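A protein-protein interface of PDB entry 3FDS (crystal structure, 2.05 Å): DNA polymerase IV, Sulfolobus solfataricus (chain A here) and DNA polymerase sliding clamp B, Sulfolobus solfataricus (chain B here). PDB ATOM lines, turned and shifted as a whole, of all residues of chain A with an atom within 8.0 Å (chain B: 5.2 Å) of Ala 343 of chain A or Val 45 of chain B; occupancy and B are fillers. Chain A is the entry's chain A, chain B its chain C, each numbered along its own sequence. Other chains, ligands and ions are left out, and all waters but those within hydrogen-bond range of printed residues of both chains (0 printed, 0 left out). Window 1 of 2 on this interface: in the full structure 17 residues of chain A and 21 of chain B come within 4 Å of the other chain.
Hydrophobic or aromatic side chains of chain A that line the printed part of chain B: Ile 341, Ala 343 and Leu 346.
Among the printed residues, 12 pairs touch across the chains.
Among the printed residues, no Asp or Glu carboxylate lies within 4 Å of a Lys or Arg side-chain nitrogen of the other chain.
Lys 278 of chain A touches none of the printed residues of chain B.
Ile 280 of chain A touches none of the printed residues of chain B.
Ala 343 of chain A touches just one residue of chain B: Val 45 (3.6 Å).
Printed residues of chain A within 4 Å of Trp 244 of chain B: Leu 346.
Printed residues of chain A within 4 Å of Ile 245 of chain B: Leu 346 (3.97 Å).
The nearest residue of chain B that does not touch Ala 343 of chain A is Arg 248 of chain B (4.7 Å).
Among the printed residues, pairs that only touch across the chains: Ile 344 of chain A with Ala 246 of chain B, Leu 346 of chain A with Met 47 of chain B, Ile 341 of chain A with Arg 248 of chain B, Leu 346 of chain A with Ala 246 of chain B, Leu 346 of chain A with Trp 244 of chain B, Ala 343 of chain A with Val 45 of chain B, Leu 346 of chain A with Val 45 of chain B, Asp 347 of chain A with Lys 44 of chain B, Gly 345 of chain A with Lys 44 of chain B, Glu 342 of chain A with Arg 248 of chain B and Leu 346 of chain A with Ile 245 of chain B.
The backbone NH (N) of Ile 341 of chain A sits at hydrogen-bond distance from the backbone carbonyl oxygen (O) of Ile 280 of chain A (2.7 Å).
N of Val 45 of chain B sits at hydrogen-bond distance from OG1 of Thr 41 of chain B (3.4 Å).
The side-chain carboxylate (OD1) of Asp 43 of chain B sits at hydrogen-bond distance from the backbone NH (N) of Val 45 of chain B (3.0 Å).
The backbone NH (N) of Ala 246 of chain B sits at hydrogen-bond distance from the backbone carbonyl oxygen (O) of Val 45 of chain B, at 2.8 Å.
N of Met 47 of chain B is in hydrogen-bond range of O of Trp 244 of chain B (2.9 Å).
The backbone NH (N) of Leu 346 of chain A is in hydrogen-bond range of the backbone carbonyl oxygen (O) of Lys 44 of chain B, 2.8 Å away.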
ATOM      1  N   LYS A 278     -24.237   3.774  -4.417  1.00  0.00           N
ATOM      2  CA  LYS A 278     -23.287   2.985  -3.655  1.00  0.00           C
ATOM      3  C   LYS A 278     -21.792   3.304  -3.935  1.00  0.00           C
ATOM      4  O   LYS A 278     -20.914   2.847  -3.185  1.00  0.00           O
ATOM      5  CB  LYS A 278     -23.603   1.471  -3.838  1.00  0.00           C
ATOM      6  CG  LYS A 278     -23.468   0.888  -5.303  1.00  0.00           C
ATOM      7  CD  LYS A 278     -24.075   1.832  -6.414  1.00  0.00           C
ATOM      8  CE  LYS A 278     -23.806   1.347  -7.852  1.00  0.00           C
ATOM      9  NZ  LYS A 278     -23.929   2.497  -8.819  1.00  0.00           N
ATOM     10  N   ARG A 279     -21.523   4.089  -4.983  1.00  0.00           N
ATOM     11  CA  ARG A 279     -20.160   4.468  -5.359  1.00  0.00           C
ATOM     12  C   ARG A 279     -19.658   5.585  -4.494  1.00  0.00           C
ATOM     13  O   ARG A 279     -20.295   6.638  -4.388  1.00  0.00           O
ATOM     14  CB  ARG A 279     -20.118   4.952  -6.800  1.00  0.00           C
ATOM     15  CG  ARG A 279     -20.038   3.850  -7.834  1.00  0.00           C
ATOM     16  CD  ARG A 279     -20.378   4.429  -9.199  1.00  0.00           C
ATOM     17  NE  ARG A 279     -21.759   4.879  -9.234  1.00  0.00           N
ATOM     18  CZ  ARG A 279     -22.472   4.987 -10.345  1.00  0.00           C
ATOM     19  NH1 ARG A 279     -21.926   4.690 -11.512  1.00  0.00           N
ATOM     20  NH2 ARG A 279     -23.728   5.398 -10.290  1.00  0.00           N
ATOM     21  N   ILE A 280     -18.487   5.378  -3.907  1.00  0.00           N
ATOM     22  CA  ILE A 280     -17.860   6.395  -3.106  1.00  0.00           C
ATOM     23  C   ILE A 280     -16.727   7.044  -3.923  1.00  0.00           C
ATOM     24  O   ILE A 280     -15.753   6.365  -4.240  1.00  0.00           O
ATOM     25  CB  ILE A 280     -17.292   5.791  -1.792  1.00  0.00           C
ATOM     26  CG1 ILE A 280     -18.394   5.056  -1.004  1.00  0.00           C
ATOM     27  CG2 ILE A 280     -16.653   6.881  -0.947  1.00  0.00           C
ATOM     28  CD1 ILE A 280     -17.893   4.377   0.311  1.00  0.00           C
ATOM     29  N   PHE A 340     -13.835   6.085  -8.308  1.00  0.00           N
ATOM     30  CA  PHE A 340     -14.802   5.489  -7.408  1.00  0.00           C
ATOM     31  C   PHE A 340     -14.268   4.294  -6.647  1.00  0.00           C
ATOM     32  O   PHE A 340     -13.522   3.459  -7.181  1.00  0.00           O
ATOM     33  CB  PHE A 340     -16.029   5.060  -8.219  1.00  0.00           C
ATOM     34  CG  PHE A 340     -16.690   6.203  -8.963  1.00  0.00           C
ATOM     35  CD1 PHE A 340     -17.050   7.350  -8.310  1.00  0.00           C
ATOM     36  CD2 PHE A 340     -16.961   6.096 -10.334  1.00  0.00           C
ATOM     37  CE1 PHE A 340     -17.692   8.441  -9.008  1.00  0.00           C
ATOM     38  CE2 PHE A 340     -17.590   7.168 -11.033  1.00  0.00           C
ATOM     39  CZ  PHE A 340     -17.968   8.323 -10.379  1.00  0.00           C
ATOM     40  N   ILE A 341     -14.698   4.184  -5.387  1.00  0.00           N
ATOM     41  CA  ILE A 341     -14.458   2.966  -4.614  1.00  0.00           C
ATOM     42  C   ILE A 341     -15.775   2.191  -4.712  1.00  0.00           C
ATOM     43  O   ILE A 341     -16.830   2.689  -4.271  1.00  0.00           O
ATOM     44  CB  ILE A 341     -14.154   3.306  -3.123  1.00  0.00           C
ATOM     45  CG1 ILE A 341     -12.849   4.136  -3.018  1.00  0.00           C
ATOM     46  CG2 ILE A 341     -14.144   2.025  -2.251  1.00  0.00           C
ATOM     47  CD1 ILE A 341     -12.614   4.796  -1.650  1.00  0.00           C
ATOM     48  N   GLU A 342     -15.744   1.016  -5.317  1.00  0.00           N
ATOM     49  CA  GLU A 342     -16.974   0.236  -5.368  1.00  0.00           C
ATOM     50  C   GLU A 342     -16.811  -1.164  -4.782  1.00  0.00           C
ATOM     51  O   GLU A 342     -16.124  -2.023  -5.338  1.00  0.00           O
ATOM     52  CB  GLU A 342     -17.632   0.234  -6.741  1.00  0.00           C
ATOM     53  CG  GLU A 342     -19.066  -0.257  -6.617  1.00  0.00           C
ATOM     54  CD  GLU A 342     -19.875   0.014  -7.820  1.00  0.00           C
ATOM     55  OE1 GLU A 342     -19.330   0.635  -8.766  1.00  0.00           O
ATOM     56  OE2 GLU A 342     -21.068  -0.381  -7.821  1.00  0.00           O
ATOM     57  N   ALA A 343     -17.406  -1.322  -3.613  1.00  0.00           N
ATOM     58  CA  ALA A 343     -17.375  -2.543  -2.853  1.00  0.00           C
ATOM     59  C   ALA A 343     -18.441  -3.482  -3.394  1.00  0.00           C
ATOM     60  O   ALA A 343     -19.539  -3.063  -3.734  1.00  0.00           O
ATOM     61  CB  ALA A 343     -17.666  -2.228  -1.409  1.00  0.00           C
ATOM     62  N   ILE A 344     -18.102  -4.754  -3.503  1.00  0.00           N
ATOM     63  CA  ILE A 344     -19.096  -5.748  -3.830  1.00  0.00           C
ATOM     64  C   ILE A 344     -19.198  -6.709  -2.632  1.00  0.00           C
ATOM     65  O   ILE A 344     -18.188  -7.001  -1.976  1.00  0.00           O
ATOM     66  CB  ILE A 344     -18.748  -6.427  -5.148  1.00  0.00           C
ATOM     67  CG1 ILE A 344     -17.530  -7.292  -4.973  1.00  0.00           C
ATOM     68  CG2 ILE A 344     -18.426  -5.363  -6.261  1.00  0.00           C
ATOM     69  CD1 ILE A 344     -17.632  -8.459  -5.843  1.00  0.00           C
ATOM     70  N   GLY A 345     -20.410  -7.128  -2.299  1.00  0.00           N
ATOM     71  CA  GLY A 345     -20.618  -7.956  -1.104  1.00  0.00           C
ATOM     72  C   GLY A 345     -20.171  -9.393  -1.318  1.00  0.00           C
ATOM     73  O   GLY A 345     -20.169  -9.905  -2.465  1.00  0.00           O
ATOM     74  N   LEU A 346     -19.831 -10.064  -0.219  1.00  0.00           N
ATOM     75  CA  LEU A 346     -19.416 -11.473  -0.261  1.00  0.00           C
ATOM     76  C   LEU A 346     -20.533 -12.373  -0.785  1.00  0.00           C
ATOM     77  O   LEU A 346     -20.270 -13.474  -1.280  1.00  0.00           O
ATOM     78  CB  LEU A 346     -18.964 -11.966   1.108  1.00  0.00           C
ATOM     79  CG  LEU A 346     -17.556 -11.527   1.518  1.00  0.00           C
ATOM     80  CD1 LEU A 346     -17.365 -11.838   3.000  1.00  0.00           C
ATOM     81  CD2 LEU A 346     -16.538 -12.245   0.705  1.00  0.00           C
ATOM     82  N   ASP A 347     -21.765 -11.898  -0.609  1.00  0.00           N
ATOM     83  CA  ASP A 347     -22.884 -12.232  -1.520  1.00  0.00           C
ATOM     84  C   ASP A 347     -22.401 -13.072  -2.703  1.00  0.00           C
ATOM     85  O   ASP A 347     -22.986 -14.136  -2.917  1.00  0.00           O
ATOM     86  CB  ASP A 347     -23.594 -10.949  -1.919  1.00  0.00           C
ATOM     87  CG  ASP A 347     -24.655 -10.657  -0.965  1.00  0.00           C
ATOM     88  OD1 ASP A 347     -24.864 -11.589  -0.161  1.00  0.00           O
ATOM     89  OD2 ASP A 347     -25.258  -9.571  -0.993  1.00  0.00           O
ATOM     90  N   LYS A 348     -21.508 -12.539  -3.588  1.00  0.00           N
ATOM     91  CA  LYS A 348     -21.996 -12.502  -5.015  1.00  0.00           C
ATOM     92  C   LYS A 348     -21.229 -13.802  -5.256  1.00  0.00           C
ATOM     93  O   LYS A 348     -21.132 -14.300  -6.359  1.00  0.00           O
ATOM     94  CB  LYS A 348     -21.351 -11.385  -5.829  1.00  0.00           C
ATOM     95  CG  LYS A 348     -21.819  -9.945  -5.559  1.00  0.00           C
ATOM     96  CD  LYS A 348     -22.911  -9.878  -4.540  1.00  0.00           C
ATOM     97  CE  LYS A 348     -23.896  -8.777  -4.843  1.00  0.00           C
ATOM     98  NZ  LYS A 348     -25.061  -9.349  -5.545  1.00  0.00           N
ATOM     99  N   THR B  41     -19.892  -7.737   8.178  1.00  0.00           N
ATOM    100  CA  THR B  41     -20.061  -6.293   8.295  1.00  0.00           C
ATOM    101  C   THR B  41     -21.279  -5.866   7.497  1.00  0.00           C
ATOM    102  O   THR B  41     -21.754  -6.581   6.596  1.00  0.00           O
ATOM    103  CB  THR B  41     -18.837  -5.534   7.731  1.00  0.00           C
ATOM    104  OG1 THR B  41     -18.592  -5.968   6.387  1.00  0.00           O
ATOM    105  CG2 THR B  41     -17.592  -5.826   8.562  1.00  0.00           C
ATOM    106  N   ASP B  43     -21.729  -3.747   5.075  1.00  0.00           N
ATOM    107  CA  ASP B  43     -21.544  -3.714   3.615  1.00  0.00           C
ATOM    108  C   ASP B  43     -21.243  -5.103   3.033  1.00  0.00           C
ATOM    109  O   ASP B  43     -21.040  -5.243   1.844  1.00  0.00           O
ATOM    110  CB  ASP B  43     -20.459  -2.699   3.239  1.00  0.00           C
ATOM    111  CG  ASP B  43     -19.084  -3.037   3.816  1.00  0.00           C
ATOM    112  OD1 ASP B  43     -18.868  -4.125   4.375  1.00  0.00           O
ATOM    113  OD2 ASP B  43     -18.154  -2.196   3.702  1.00  0.00           O
ATOM    114  N   LYS B  44     -21.162  -6.116   3.896  1.00  0.00           N
ATOM    115  CA  LYS B  44     -20.955  -7.513   3.477  1.00  0.00           C
ATOM    116  C   LYS B  44     -19.555  -7.739   2.881  1.00  0.00           C
ATOM    117  O   LYS B  44     -19.322  -8.746   2.202  1.00  0.00           O
ATOM    118  CB  LYS B  44     -22.076  -7.950   2.474  1.00  0.00           C
ATOM    119  CG  LYS B  44     -23.400  -8.383   3.181  1.00  0.00           C
ATOM    120  CD  LYS B  44     -24.627  -8.169   2.300  1.00  0.00           C
ATOM    121  CE  LYS B  44     -25.932  -8.575   3.008  1.00  0.00           C
ATOM    122  NZ  LYS B  44     -25.895  -8.333   4.498  1.00  0.00           N
ATOM    123  N   VAL B  45     -18.618  -6.815   3.094  1.00  0.00           N
ATOM    124  CA  VAL B  45     -17.303  -7.050   2.477  1.00  0.00           C
ATOM    125  C   VAL B  45     -16.427  -7.978   3.332  1.00  0.00           C
ATOM    126  O   VAL B  45     -15.584  -8.683   2.796  1.00  0.00           O
ATOM    127  CB  VAL B  45     -16.554  -5.806   1.805  1.00  0.00           C
ATOM    128  CG1 VAL B  45     -17.461  -4.637   1.287  1.00  0.00           C
ATOM    129  CG2 VAL B  45     -15.290  -5.421   2.478  1.00  0.00           C
ATOM    130  N   LEU B  46     -16.669  -8.016   4.648  1.00  0.00           N
ATOM    131  CA  LEU B  46     -15.833  -8.802   5.549  1.00  0.00           C
ATOM    132  C   LEU B  46     -16.686  -9.758   6.375  1.00  0.00           C
ATOM    133  O   LEU B  46     -17.690  -9.356   6.926  1.00  0.00           O
ATOM    134  CB  LEU B  46     -14.950  -7.893   6.455  1.00  0.00           C
ATOM    135  CG  LEU B  46     -14.060  -8.532   7.555  1.00  0.00           C
ATOM    136  CD1 LEU B  46     -12.866  -9.311   6.904  1.00  0.00           C
ATOM    137  CD2 LEU B  46     -13.508  -7.461   8.592  1.00  0.00           C
ATOM    138  N   MET B  47     -16.293 -11.033   6.402  1.00  0.00           N
ATOM    139  CA  MET B  47     -16.969 -12.060   7.192  1.00  0.00           C
ATOM    140  C   MET B  47     -16.008 -12.695   8.192  1.00  0.00           C
ATOM    141  O   MET B  47     -14.869 -12.971   7.846  1.00  0.00           O
ATOM    142  CB  MET B  47     -17.496 -13.147   6.255  1.00  0.00           C
ATOM    143  CG  MET B  47     -18.350 -14.216   6.938  1.00  0.00           C
ATOM    144  SD  MET B  47     -18.666 -15.555   5.772  1.00  0.00           S
ATOM    145  CE  MET B  47     -20.081 -14.961   4.841  1.00  0.00           C
ATOM    146  N   SER B 201     -10.001  -3.818   0.310  1.00  0.00           N
ATOM    147  CA  SER B 201      -9.955  -2.792   1.327  1.00  0.00           C
ATOM    148  C   SER B 201      -8.820  -3.067   2.304  1.00  0.00           C
ATOM    149  O   SER B 201      -8.771  -4.114   2.888  1.00  0.00           O
ATOM    150  CB  SER B 201     -11.268  -2.750   2.081  1.00  0.00           C
ATOM    151  OG  SER B 201     -11.092  -1.965   3.210  1.00  0.00           O
ATOM    152  N   MET B 204     -10.303  -3.424   5.891  1.00  0.00           N
ATOM    153  CA  MET B 204     -10.870  -4.746   6.131  1.00  0.00           C
ATOM    154  C   MET B 204      -9.758  -5.790   6.306  1.00  0.00           C
ATOM    155  O   MET B 204      -9.901  -6.706   7.120  1.00  0.00           O
ATOM    156  CB  MET B 204     -11.809  -5.182   5.016  1.00  0.00           C
ATOM    157  CG  MET B 204     -13.132  -4.369   4.885  1.00  0.00           C
ATOM    158  SD  MET B 204     -14.150  -4.237   6.348  1.00  0.00           S
ATOM    159  CE  MET B 204     -13.481  -2.805   7.185  1.00  0.00           C
ATOM    160  N   TRP B 244     -13.183 -13.913   5.587  1.00  0.00           N
ATOM    161  CA  TRP B 244     -13.283 -13.758   4.147  1.00  0.00           C
ATOM    162  C   TRP B 244     -13.378 -12.253   3.854  1.00  0.00           C
ATOM    163  O   TRP B 244     -14.113 -11.547   4.539  1.00  0.00           O
ATOM    164  CB  TRP B 244     -14.556 -14.369   3.627  1.00  0.00           C
ATOM    165  CG  TRP B 244     -14.581 -15.889   3.589  1.00  0.00           C
ATOM    166  CD1 TRP B 244     -15.086 -16.718   4.539  1.00  0.00           C
ATOM    167  CD2 TRP B 244     -14.070 -16.727   2.555  1.00  0.00           C
ATOM    168  NE1 TRP B 244     -14.972 -18.034   4.147  1.00  0.00           N
ATOM    169  CE2 TRP B 244     -14.333 -18.066   2.931  1.00  0.00           C
ATOM    170  CE3 TRP B 244     -13.438 -16.481   1.331  1.00  0.00           C
ATOM    171  CZ2 TRP B 244     -13.975 -19.153   2.136  1.00  0.00           C
ATOM    172  CZ3 TRP B 244     -13.092 -17.578   0.519  1.00  0.00           C
ATOM    173  CH2 TRP B 244     -13.363 -18.896   0.938  1.00  0.00           C
ATOM    174  N   ILE B 245     -12.709 -11.810   2.791  1.00  0.00           N
ATOM    175  CA  ILE B 245     -12.725 -10.404   2.348  1.00  0.00           C
ATOM    176  C   ILE B 245     -13.069 -10.332   0.882  1.00  0.00           C
ATOM    177  O   ILE B 245     -12.388 -10.925   0.061  1.00  0.00           O
ATOM    178  CB  ILE B 245     -11.359  -9.742   2.530  1.00  0.00           C
ATOM    179  CG1 ILE B 245     -10.734 -10.156   3.900  1.00  0.00           C
ATOM    180  CG2 ILE B 245     -11.484  -8.206   2.408  1.00  0.00           C
ATOM    181  CD1 ILE B 245      -9.273  -9.469   4.121  1.00  0.00           C
ATOM    182  N   ALA B 246     -14.135  -9.597   0.559  1.00  0.00           N
ATOM    183  CA  ALA B 246     -14.610  -9.499  -0.825  1.00  0.00           C
ATOM    184  C   ALA B 246     -13.614  -8.649  -1.601  1.00  0.00           C
ATOM    185  O   ALA B 246     -13.022  -7.729  -1.037  1.00  0.00           O
ATOM    186  CB  ALA B 246     -16.012  -8.914  -0.884  1.00  0.00           C
ATOM    187  N   ARG B 248     -12.274  -5.932  -4.613  1.00  0.00           N
ATOM    188  CA  ARG B 248     -12.677  -4.745  -5.402  1.00  0.00           C
ATOM    189  C   ARG B 248     -12.695  -5.149  -6.870  1.00  0.00           C
ATOM    190  O   ARG B 248     -11.707  -5.680  -7.422  1.00  0.00           O
ATOM    191  CB  ARG B 248     -11.671  -3.600  -5.205  1.00  0.00           C
ATOM    192  CG  ARG B 248     -11.568  -3.115  -3.733  1.00  0.00           C
ATOM    193  CD  ARG B 248     -12.621  -2.087  -3.491  1.00  0.00           C
ATOM    194  NE  ARG B 248     -12.818  -1.686  -2.100  1.00  0.00           N
ATOM    195  CZ  ARG B 248     -12.096  -0.785  -1.455  1.00  0.00           C
ATOM    196  NH1 ARG B 248     -11.049  -0.206  -2.057  1.00  0.00           N
ATOM    197  NH2 ARG B 248     -12.415  -0.475  -0.184  1.00  0.00           N
